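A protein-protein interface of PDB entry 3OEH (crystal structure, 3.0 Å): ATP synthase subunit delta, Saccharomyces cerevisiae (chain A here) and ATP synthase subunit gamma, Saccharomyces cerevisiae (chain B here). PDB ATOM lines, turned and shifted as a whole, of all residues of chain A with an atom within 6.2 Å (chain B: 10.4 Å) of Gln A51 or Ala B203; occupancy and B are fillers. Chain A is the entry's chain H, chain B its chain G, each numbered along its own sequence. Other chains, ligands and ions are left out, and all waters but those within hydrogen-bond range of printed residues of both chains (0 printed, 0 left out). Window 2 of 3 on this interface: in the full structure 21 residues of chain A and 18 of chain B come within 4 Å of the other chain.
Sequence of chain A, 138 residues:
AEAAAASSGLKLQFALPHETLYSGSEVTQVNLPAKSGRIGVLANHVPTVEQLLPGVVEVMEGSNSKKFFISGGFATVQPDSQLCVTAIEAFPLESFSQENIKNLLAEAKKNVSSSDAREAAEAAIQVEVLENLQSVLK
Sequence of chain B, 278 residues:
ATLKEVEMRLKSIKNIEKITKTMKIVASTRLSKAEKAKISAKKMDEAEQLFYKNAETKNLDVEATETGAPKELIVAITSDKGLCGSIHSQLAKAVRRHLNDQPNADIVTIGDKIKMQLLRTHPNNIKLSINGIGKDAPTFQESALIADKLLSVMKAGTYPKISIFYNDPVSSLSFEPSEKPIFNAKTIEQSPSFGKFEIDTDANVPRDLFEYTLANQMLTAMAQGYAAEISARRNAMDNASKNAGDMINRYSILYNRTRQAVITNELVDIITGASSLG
OE1 of Gln A51 sits close to OD2 of Asp B208, at 2.9 Å.
N of Leu A52 lies within hydrogen-bond range of O of Gly A73, at 2.5 Å.
Among the printed residues, merely in contact across the chains: Gln A51 with Val B205 (3.4 Å), Phe A74 with Leu B209 (3.5 Å), Val A49 with Val B205 (3.7 Å), Gln A51 with Ala B203 (3.8 Å), Phe A74 with Asp B208 (3.8 Å), Val A49 with Leu B209 (3.9 Å), Gly A73 with Tyr B212 (3.9 Å), Phe A74 with Tyr B212 (3.9 Å) and Phe A74 with Val B205 (3.9 Å).
Of the printed residues of chain B, Val A49 touches Val B205 (3.7 Å) and Leu B209 (3.9 Å).
No residue of chain B comes within 4 Å of Leu A53.
Of chain B, only Val B205, Asp B208, Leu B209 and Tyr B212 come within 4 Å of Phe A74.
No residue of chain B comes within 4 Å of Ala A75.
Ile B199 touches none of the printed residues of chain A.
Ala B203 touches just one residue of chain A: Gln A51 (3.8 Å).
Of the printed residues of chain A, Val B205 touches Val A49, Gln A51 and Phe A74.
Of the printed residues of chain A, Tyr B212 touches Gly A73 and Phe A74.
Printed residues of chain A that touch a printed residue of chain B: Val A49, Gln A51, Gly A73 and Phe A74.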
ATOM      1  N   PRO A  33       5.607  -3.359 -18.868  1.00  0.00           N
ATOM      2  CA  PRO A  33       6.306  -2.772 -17.723  1.00  0.00           C
ATOM      3  C   PRO A  33       6.091  -1.260 -17.634  1.00  0.00           C
ATOM      4  O   PRO A  33       6.697  -0.508 -18.394  1.00  0.00           O
ATOM      5  CB  PRO A  33       7.771  -3.087 -18.009  1.00  0.00           C
ATOM      6  CG  PRO A  33       7.858  -3.226 -19.494  1.00  0.00           C
ATOM      7  CD  PRO A  33       6.490  -3.508 -20.037  1.00  0.00           C
ATOM      8  N   ALA A  34       5.239  -0.826 -16.707  1.00  0.00           N
ATOM      9  CA  ALA A  34       4.842   0.585 -16.593  1.00  0.00           C
ATOM     10  C   ALA A  34       5.754   1.417 -15.670  1.00  0.00           C
ATOM     11  O   ALA A  34       6.976   1.215 -15.638  1.00  0.00           O
ATOM     12  CB  ALA A  34       3.371   0.687 -16.155  1.00  0.00           C
ATOM     13  N   LYS A  35       5.147   2.355 -14.939  1.00  0.00           N
ATOM     14  CA  LYS A  35       5.839   3.215 -13.966  1.00  0.00           C
ATOM     15  C   LYS A  35       6.604   2.402 -12.904  1.00  0.00           C
ATOM     16  O   LYS A  35       7.689   2.796 -12.465  1.00  0.00           O
ATOM     17  CB  LYS A  35       4.844   4.199 -13.316  1.00  0.00           C
ATOM     18  CG  LYS A  35       3.804   3.578 -12.360  1.00  0.00           C
ATOM     19  CD  LYS A  35       2.706   2.824 -13.099  1.00  0.00           C
ATOM     20  CE  LYS A  35       2.224   1.638 -12.283  1.00  0.00           C
ATOM     21  NZ  LYS A  35       1.596   0.593 -13.141  1.00  0.00           N
ATOM     22  N   VAL A  49      -2.618   6.524 -20.096  1.00  0.00           N
ATOM     23  CA  VAL A  49      -1.281   6.796 -20.640  1.00  0.00           C
ATOM     24  C   VAL A  49      -0.214   6.463 -19.591  1.00  0.00           C
ATOM     25  O   VAL A  49      -0.186   7.057 -18.515  1.00  0.00           O
ATOM     26  CB  VAL A  49      -1.101   8.254 -21.144  1.00  0.00           C
ATOM     27  CG1 VAL A  49       0.330   8.487 -21.589  1.00  0.00           C
ATOM     28  CG2 VAL A  49      -2.037   8.542 -22.296  1.00  0.00           C
ATOM     29  N   GLU A  50       0.649   5.502 -19.919  1.00  0.00           N
ATOM     30  CA  GLU A  50       1.759   5.115 -19.052  1.00  0.00           C
ATOM     31  C   GLU A  50       3.060   5.023 -19.831  1.00  0.00           C
ATOM     32  O   GLU A  50       3.091   4.571 -20.974  1.00  0.00           O
ATOM     33  CB  GLU A  50       1.476   3.782 -18.353  1.00  0.00           C
ATOM     34  N   GLN A  51       4.133   5.471 -19.198  1.00  0.00           N
ATOM     35  CA  GLN A  51       5.459   5.360 -19.763  1.00  0.00           C
ATOM     36  C   GLN A  51       5.937   3.947 -19.516  1.00  0.00           C
ATOM     37  O   GLN A  51       5.708   3.384 -18.442  1.00  0.00           O
ATOM     38  CB  GLN A  51       6.400   6.336 -19.072  1.00  0.00           C
ATOM     39  CG  GLN A  51       5.780   7.680 -18.833  1.00  0.00           C
ATOM     40  CD  GLN A  51       6.136   8.257 -17.494  1.00  0.00           C
ATOM     41  OE1 GLN A  51       7.307   8.307 -17.123  1.00  0.00           O
ATOM     42  NE2 GLN A  51       5.126   8.710 -16.757  1.00  0.00           N
ATOM     43  N   LEU A  52       6.590   3.372 -20.516  1.00  0.00           N
ATOM     44  CA  LEU A  52       7.231   2.073 -20.369  1.00  0.00           C
ATOM     45  C   LEU A  52       8.685   2.250 -19.936  1.00  0.00           C
ATOM     46  O   LEU A  52       9.442   3.004 -20.560  1.00  0.00           O
ATOM     47  CB  LEU A  52       7.165   1.277 -21.677  1.00  0.00           C
ATOM     48  CG  LEU A  52       5.793   0.926 -22.254  1.00  0.00           C
ATOM     49  CD1 LEU A  52       5.954   0.351 -23.643  1.00  0.00           C
ATOM     50  CD2 LEU A  52       5.037  -0.032 -21.360  1.00  0.00           C
ATOM     51  N   LEU A  53       9.053   1.565 -18.854  1.00  0.00           N
ATOM     52  CA  LEU A  53      10.446   1.432 -18.442  1.00  0.00           C
ATOM     53  C   LEU A  53      11.130   0.397 -19.364  1.00  0.00           C
ATOM     54  O   LEU A  53      10.475  -0.172 -20.250  1.00  0.00           O
ATOM     55  CB  LEU A  53      10.513   1.018 -16.967  1.00  0.00           C
ATOM     56  N   GLY A  73       9.675   3.557 -23.564  1.00  0.00           N
ATOM     57  CA  GLY A  73       8.743   4.325 -24.363  1.00  0.00           C
ATOM     58  C   GLY A  73       7.448   4.530 -23.628  1.00  0.00           C
ATOM     59  O   GLY A  73       7.453   4.796 -22.430  1.00  0.00           O
ATOM     60  N   PHE A  74       6.346   4.385 -24.356  1.00  0.00           N
ATOM     61  CA  PHE A  74       5.029   4.762 -23.873  1.00  0.00           C
ATOM     62  C   PHE A  74       3.969   3.777 -24.322  1.00  0.00           C
ATOM     63  O   PHE A  74       3.967   3.335 -25.472  1.00  0.00           O
ATOM     64  CB  PHE A  74       4.653   6.143 -24.406  1.00  0.00           C
ATOM     65  CG  PHE A  74       4.958   7.268 -23.467  1.00  0.00           C
ATOM     66  CD1 PHE A  74       6.193   7.903 -23.497  1.00  0.00           C
ATOM     67  CD2 PHE A  74       3.994   7.715 -22.569  1.00  0.00           C
ATOM     68  CE1 PHE A  74       6.476   8.962 -22.632  1.00  0.00           C
ATOM     69  CE2 PHE A  74       4.260   8.778 -21.702  1.00  0.00           C
ATOM     70  CZ  PHE A  74       5.507   9.404 -21.735  1.00  0.00           C
ATOM     71  N   ALA A  75       3.067   3.448 -23.402  1.00  0.00           N
ATOM     72  CA  ALA A  75       1.861   2.701 -23.726  1.00  0.00           C
ATOM     73  C   ALA A  75       0.653   3.597 -23.516  1.00  0.00           C
ATOM     74  O   ALA A  75       0.609   4.392 -22.573  1.00  0.00           O
ATOM     75  CB  ALA A  75       1.755   1.462 -22.876  1.00  0.00           C
ATOM     76  N   ALA B 185       4.702  20.339 -22.537  1.00  0.00           N
ATOM     77  CA  ALA B 185       4.011  19.725 -21.397  1.00  0.00           C
ATOM     78  C   ALA B 185       2.707  20.444 -21.079  1.00  0.00           C
ATOM     79  O   ALA B 185       1.653  19.809 -20.973  1.00  0.00           O
ATOM     80  CB  ALA B 185       4.913  19.693 -20.175  1.00  0.00           C
ATOM     81  N   GLU B 189      -1.199  18.786 -21.031  1.00  0.00           N
ATOM     82  CA  GLU B 189      -2.024  18.843 -19.810  1.00  0.00           C
ATOM     83  C   GLU B 189      -3.351  19.569 -19.986  1.00  0.00           C
ATOM     84  O   GLU B 189      -4.388  19.131 -19.484  1.00  0.00           O
ATOM     85  CB  GLU B 189      -1.277  19.577 -18.698  1.00  0.00           C
ATOM     86  CG  GLU B 189      -0.177  18.803 -18.022  1.00  0.00           C
ATOM     87  CD  GLU B 189       0.276  19.465 -16.730  1.00  0.00           C
ATOM     88  OE1 GLU B 189       0.222  20.713 -16.639  1.00  0.00           O
ATOM     89  OE2 GLU B 189       0.681  18.733 -15.799  1.00  0.00           O
ATOM     90  N   PHE B 194      -8.253  15.784 -22.481  1.00  0.00           N
ATOM     91  CA  PHE B 194      -7.188  15.106 -21.738  1.00  0.00           C
ATOM     92  C   PHE B 194      -7.742  14.152 -20.693  1.00  0.00           C
ATOM     93  O   PHE B 194      -7.176  13.082 -20.451  1.00  0.00           O
ATOM     94  CB  PHE B 194      -6.255  16.119 -21.067  1.00  0.00           C
ATOM     95  CG  PHE B 194      -5.040  15.491 -20.430  1.00  0.00           C
ATOM     96  CD1 PHE B 194      -3.924  15.177 -21.194  1.00  0.00           C
ATOM     97  CD2 PHE B 194      -5.019  15.203 -19.070  1.00  0.00           C
ATOM     98  CE1 PHE B 194      -2.807  14.592 -20.614  1.00  0.00           C
ATOM     99  CE2 PHE B 194      -3.906  14.620 -18.482  1.00  0.00           C
ATOM    100  CZ  PHE B 194      -2.796  14.315 -19.255  1.00  0.00           C
ATOM    101  N   GLU B 198      -7.176   8.125 -18.144  1.00  0.00           N
ATOM    102  CA  GLU B 198      -6.836   8.016 -16.725  1.00  0.00           C
ATOM    103  C   GLU B 198      -5.314   7.948 -16.574  1.00  0.00           C
ATOM    104  O   GLU B 198      -4.728   6.871 -16.494  1.00  0.00           O
ATOM    105  CB  GLU B 198      -7.520   6.784 -16.106  1.00  0.00           C
ATOM    106  CG  GLU B 198      -7.390   6.640 -14.580  1.00  0.00           C
ATOM    107  CD  GLU B 198      -8.329   7.560 -13.785  1.00  0.00           C
ATOM    108  OE1 GLU B 198      -8.682   8.659 -14.281  1.00  0.00           O
ATOM    109  OE2 GLU B 198      -8.709   7.183 -12.650  1.00  0.00           O
ATOM    110  N   ILE B 199      -4.682   9.117 -16.575  1.00  0.00           N
ATOM    111  CA  ILE B 199      -3.237   9.222 -16.419  1.00  0.00           C
ATOM    112  C   ILE B 199      -2.920   9.433 -14.950  1.00  0.00           C
ATOM    113  O   ILE B 199      -3.609  10.196 -14.270  1.00  0.00           O
ATOM    114  CB  ILE B 199      -2.656  10.394 -17.244  1.00  0.00           C
ATOM    115  N   ASP B 200      -1.893   8.749 -14.455  1.00  0.00           N
ATOM    116  CA  ASP B 200      -1.451   8.938 -13.076  1.00  0.00           C
ATOM    117  C   ASP B 200      -0.688  10.256 -12.973  1.00  0.00           C
ATOM    118  O   ASP B 200       0.421  10.383 -13.490  1.00  0.00           O
ATOM    119  CB  ASP B 200      -0.592   7.762 -12.613  1.00  0.00           C
ATOM    120  N   THR B 201      -1.302  11.233 -12.310  1.00  0.00           N
ATOM    121  CA  THR B 201      -0.779  12.605 -12.252  1.00  0.00           C
ATOM    122  C   THR B 201       0.398  12.795 -11.283  1.00  0.00           C
ATOM    123  O   THR B 201       0.736  13.924 -10.918  1.00  0.00           O
ATOM    124  CB  THR B 201      -1.905  13.634 -11.950  1.00  0.00           C
ATOM    125  OG1 THR B 201      -1.390  14.962 -12.100  1.00  0.00           O
ATOM    126  CG2 THR B 201      -2.474  13.456 -10.529  1.00  0.00           C
ATOM    127  N   ASP B 202       1.018  11.688 -10.886  1.00  0.00           N
ATOM    128  CA  ASP B 202       2.148  11.708  -9.960  1.00  0.00           C
ATOM    129  C   ASP B 202       3.432  12.089 -10.685  1.00  0.00           C
ATOM    130  O   ASP B 202       4.073  13.088 -10.351  1.00  0.00           O
ATOM    131  CB  ASP B 202       2.301  10.348  -9.264  1.00  0.00           C
ATOM    132  CG  ASP B 202       2.269   9.167 -10.243  1.00  0.00           C
ATOM    133  OD1 ASP B 202       1.874   9.348 -11.422  1.00  0.00           O
ATOM    134  OD2 ASP B 202       2.646   8.049  -9.823  1.00  0.00           O
ATOM    135  N   ALA B 203       3.792  11.289 -11.686  1.00  0.00           N
ATOM    136  CA  ALA B 203       4.947  11.559 -12.530  1.00  0.00           C
ATOM    137  C   ALA B 203       4.616  12.701 -13.482  1.00  0.00           C
ATOM    138  O   ALA B 203       3.503  13.243 -13.466  1.00  0.00           O
ATOM    139  CB  ALA B 203       5.344  10.302 -13.306  1.00  0.00           C
ATOM    140  N   ASN B 204       5.582  13.069 -14.311  1.00  0.00           N
ATOM    141  CA  ASN B 204       5.364  14.139 -15.255  1.00  0.00           C
ATOM    142  C   ASN B 204       5.119  13.547 -16.626  1.00  0.00           C
ATOM    143  O   ASN B 204       5.864  13.810 -17.570  1.00  0.00           O
ATOM    144  CB  ASN B 204       6.552  15.102 -15.260  1.00  0.00           C
ATOM    145  CG  ASN B 204       7.067  15.393 -13.870  1.00  0.00           C
ATOM    146  OD1 ASN B 204       7.561  14.497 -13.180  1.00  0.00           O
ATOM    147  ND2 ASN B 204       6.957  16.648 -13.445  1.00  0.00           N
ATOM    148  N   VAL B 205       4.069  12.735 -16.722  1.00  0.00           N
ATOM    149  CA  VAL B 205       3.655  12.130 -17.990  1.00  0.00           C
ATOM    150  C   VAL B 205       3.639  13.143 -19.149  1.00  0.00           C
ATOM    151  O   VAL B 205       4.157  12.834 -20.221  1.00  0.00           O
ATOM    152  CB  VAL B 205       2.284  11.420 -17.881  1.00  0.00           C
ATOM    153  CG1 VAL B 205       2.016  10.569 -19.102  1.00  0.00           C
ATOM    154  CG2 VAL B 205       2.225  10.560 -16.631  1.00  0.00           C
ATOM    155  N   PRO B 206       3.055  14.349 -18.944  1.00  0.00           N
ATOM    156  CA  PRO B 206       3.157  15.360 -19.994  1.00  0.00           C
ATOM    157  C   PRO B 206       4.593  15.768 -20.333  1.00  0.00           C
ATOM    158  O   PRO B 206       4.943  15.790 -21.517  1.00  0.00           O
ATOM    159  CB  PRO B 206       2.371  16.531 -19.417  1.00  0.00           C
ATOM    160  CG  PRO B 206       1.326  15.864 -18.587  1.00  0.00           C
ATOM    161  CD  PRO B 206       2.075  14.757 -17.918  1.00  0.00           C
ATOM    162  N   ARG B 207       5.414  16.063 -19.322  1.00  0.00           N
ATOM    163  CA  ARG B 207       6.832  16.407 -19.542  1.00  0.00           C
ATOM    164  C   ARG B 207       7.581  15.337 -20.336  1.00  0.00           C
ATOM    165  O   ARG B 207       8.284  15.648 -21.293  1.00  0.00           O
ATOM    166  CB  ARG B 207       7.543  16.667 -18.216  1.00  0.00           C
ATOM    167  CG  ARG B 207       9.060  16.736 -18.312  1.00  0.00           C
ATOM    168  CD  ARG B 207       9.699  16.196 -17.040  1.00  0.00           C
ATOM    169  NE  ARG B 207      11.147  16.380 -17.033  1.00  0.00           N
ATOM    170  CZ  ARG B 207      11.772  17.453 -16.550  1.00  0.00           C
ATOM    171  NH1 ARG B 207      11.080  18.460 -16.027  1.00  0.00           N
ATOM    172  NH2 ARG B 207      13.098  17.519 -16.595  1.00  0.00           N
ATOM    173  N   ASP B 208       7.423  14.080 -19.928  1.00  0.00           N
ATOM    174  CA  ASP B 208       8.054  12.957 -20.610  1.00  0.00           C
ATOM    175  C   ASP B 208       7.451  12.759 -21.976  1.00  0.00           C
ATOM    176  O   ASP B 208       8.169  12.548 -22.948  1.00  0.00           O
ATOM    177  CB  ASP B 208       7.912  11.678 -19.793  1.00  0.00           C
ATOM    178  CG  ASP B 208       8.806  11.669 -18.569  1.00  0.00           C
ATOM    179  OD1 ASP B 208       9.728  12.514 -18.478  1.00  0.00           O
ATOM    180  OD2 ASP B 208       8.585  10.808 -17.693  1.00  0.00           O
ATOM    181  N   LEU B 209       6.128  12.848 -22.047  1.00  0.00           N
ATOM    182  CA  LEU B 209       5.414  12.724 -23.310  1.00  0.00           C
ATOM    183  C   LEU B 209       5.875  13.762 -24.331  1.00  0.00           C
ATOM    184  O   LEU B 209       5.911  13.486 -25.521  1.00  0.00           O
ATOM    185  CB  LEU B 209       3.909  12.809 -23.079  1.00  0.00           C
ATOM    186  CG  LEU B 209       2.984  12.029 -24.013  1.00  0.00           C
ATOM    187  CD1 LEU B 209       3.643  10.783 -24.609  1.00  0.00           C
ATOM    188  CD2 LEU B 209       1.687  11.669 -23.279  1.00  0.00           C
ATOM    189  N   PHE B 210       6.253  14.944 -23.861  1.00  0.00           N
ATOM    190  CA  PHE B 210       6.773  15.980 -24.739  1.00  0.00           C
ATOM    191  C   PHE B 210       8.186  15.683 -25.224  1.00  0.00           C
ATOM    192  O   PHE B 210       8.438  15.739 -26.425  1.00  0.00           O
ATOM    193  CB  PHE B 210       6.700  17.351 -24.063  1.00  0.00           C
ATOM    194  CG  PHE B 210       7.665  18.365 -24.614  1.00  0.00           C
ATOM    195  CD1 PHE B 210       7.559  18.822 -25.924  1.00  0.00           C
ATOM    196  CD2 PHE B 210       8.669  18.882 -23.806  1.00  0.00           C
ATOM    197  CE1 PHE B 210       8.453  19.767 -26.420  1.00  0.00           C
ATOM    198  CE2 PHE B 210       9.560  19.826 -24.297  1.00  0.00           C
ATOM    199  CZ  PHE B 210       9.449  20.271 -25.601  1.00  0.00           C
ATOM    200  N   GLU B 211       9.100  15.370 -24.307  1.00  0.00           N
ATOM    201  CA  GLU B 211      10.499  15.120 -24.676  1.00  0.00           C
ATOM    202  C   GLU B 211      10.650  13.879 -25.552  1.00  0.00           C
ATOM    203  O   GLU B 211      11.516  13.816 -26.424  1.00  0.00           O
ATOM    204  CB  GLU B 211      11.375  14.990 -23.438  1.00  0.00           C
ATOM    205  CG  GLU B 211      11.308  16.191 -22.519  1.00  0.00           C
ATOM    206  CD  GLU B 211      12.380  16.184 -21.452  1.00  0.00           C
ATOM    207  OE1 GLU B 211      13.213  15.248 -21.430  1.00  0.00           O
ATOM    208  OE2 GLU B 211      12.387  17.130 -20.637  1.00  0.00           O
ATOM    209  N   TYR B 212       9.792  12.897 -25.307  1.00  0.00           N
ATOM    210  CA  TYR B 212       9.724  11.710 -26.130  1.00  0.00           C
ATOM    211  C   TYR B 212       9.224  12.080 -27.527  1.00  0.00           C
ATOM    212  O   TYR B 212       9.824  11.686 -28.521  1.00  0.00           O
ATOM    213  CB  TYR B 212       8.825  10.669 -25.464  1.00  0.00           C
ATOM    214  CG  TYR B 212       8.723   9.347 -26.187  1.00  0.00           C
ATOM    215  CD1 TYR B 212       9.751   8.409 -26.116  1.00  0.00           C
ATOM    216  CD2 TYR B 212       7.582   9.024 -26.923  1.00  0.00           C
ATOM    217  CE1 TYR B 212       9.656   7.188 -26.772  1.00  0.00           C
ATOM    218  CE2 TYR B 212       7.475   7.806 -27.582  1.00  0.00           C
ATOM    219  CZ  TYR B 212       8.517   6.894 -27.506  1.00  0.00           C
ATOM    220  OH  TYR B 212       8.418   5.689 -28.164  1.00  0.00           O
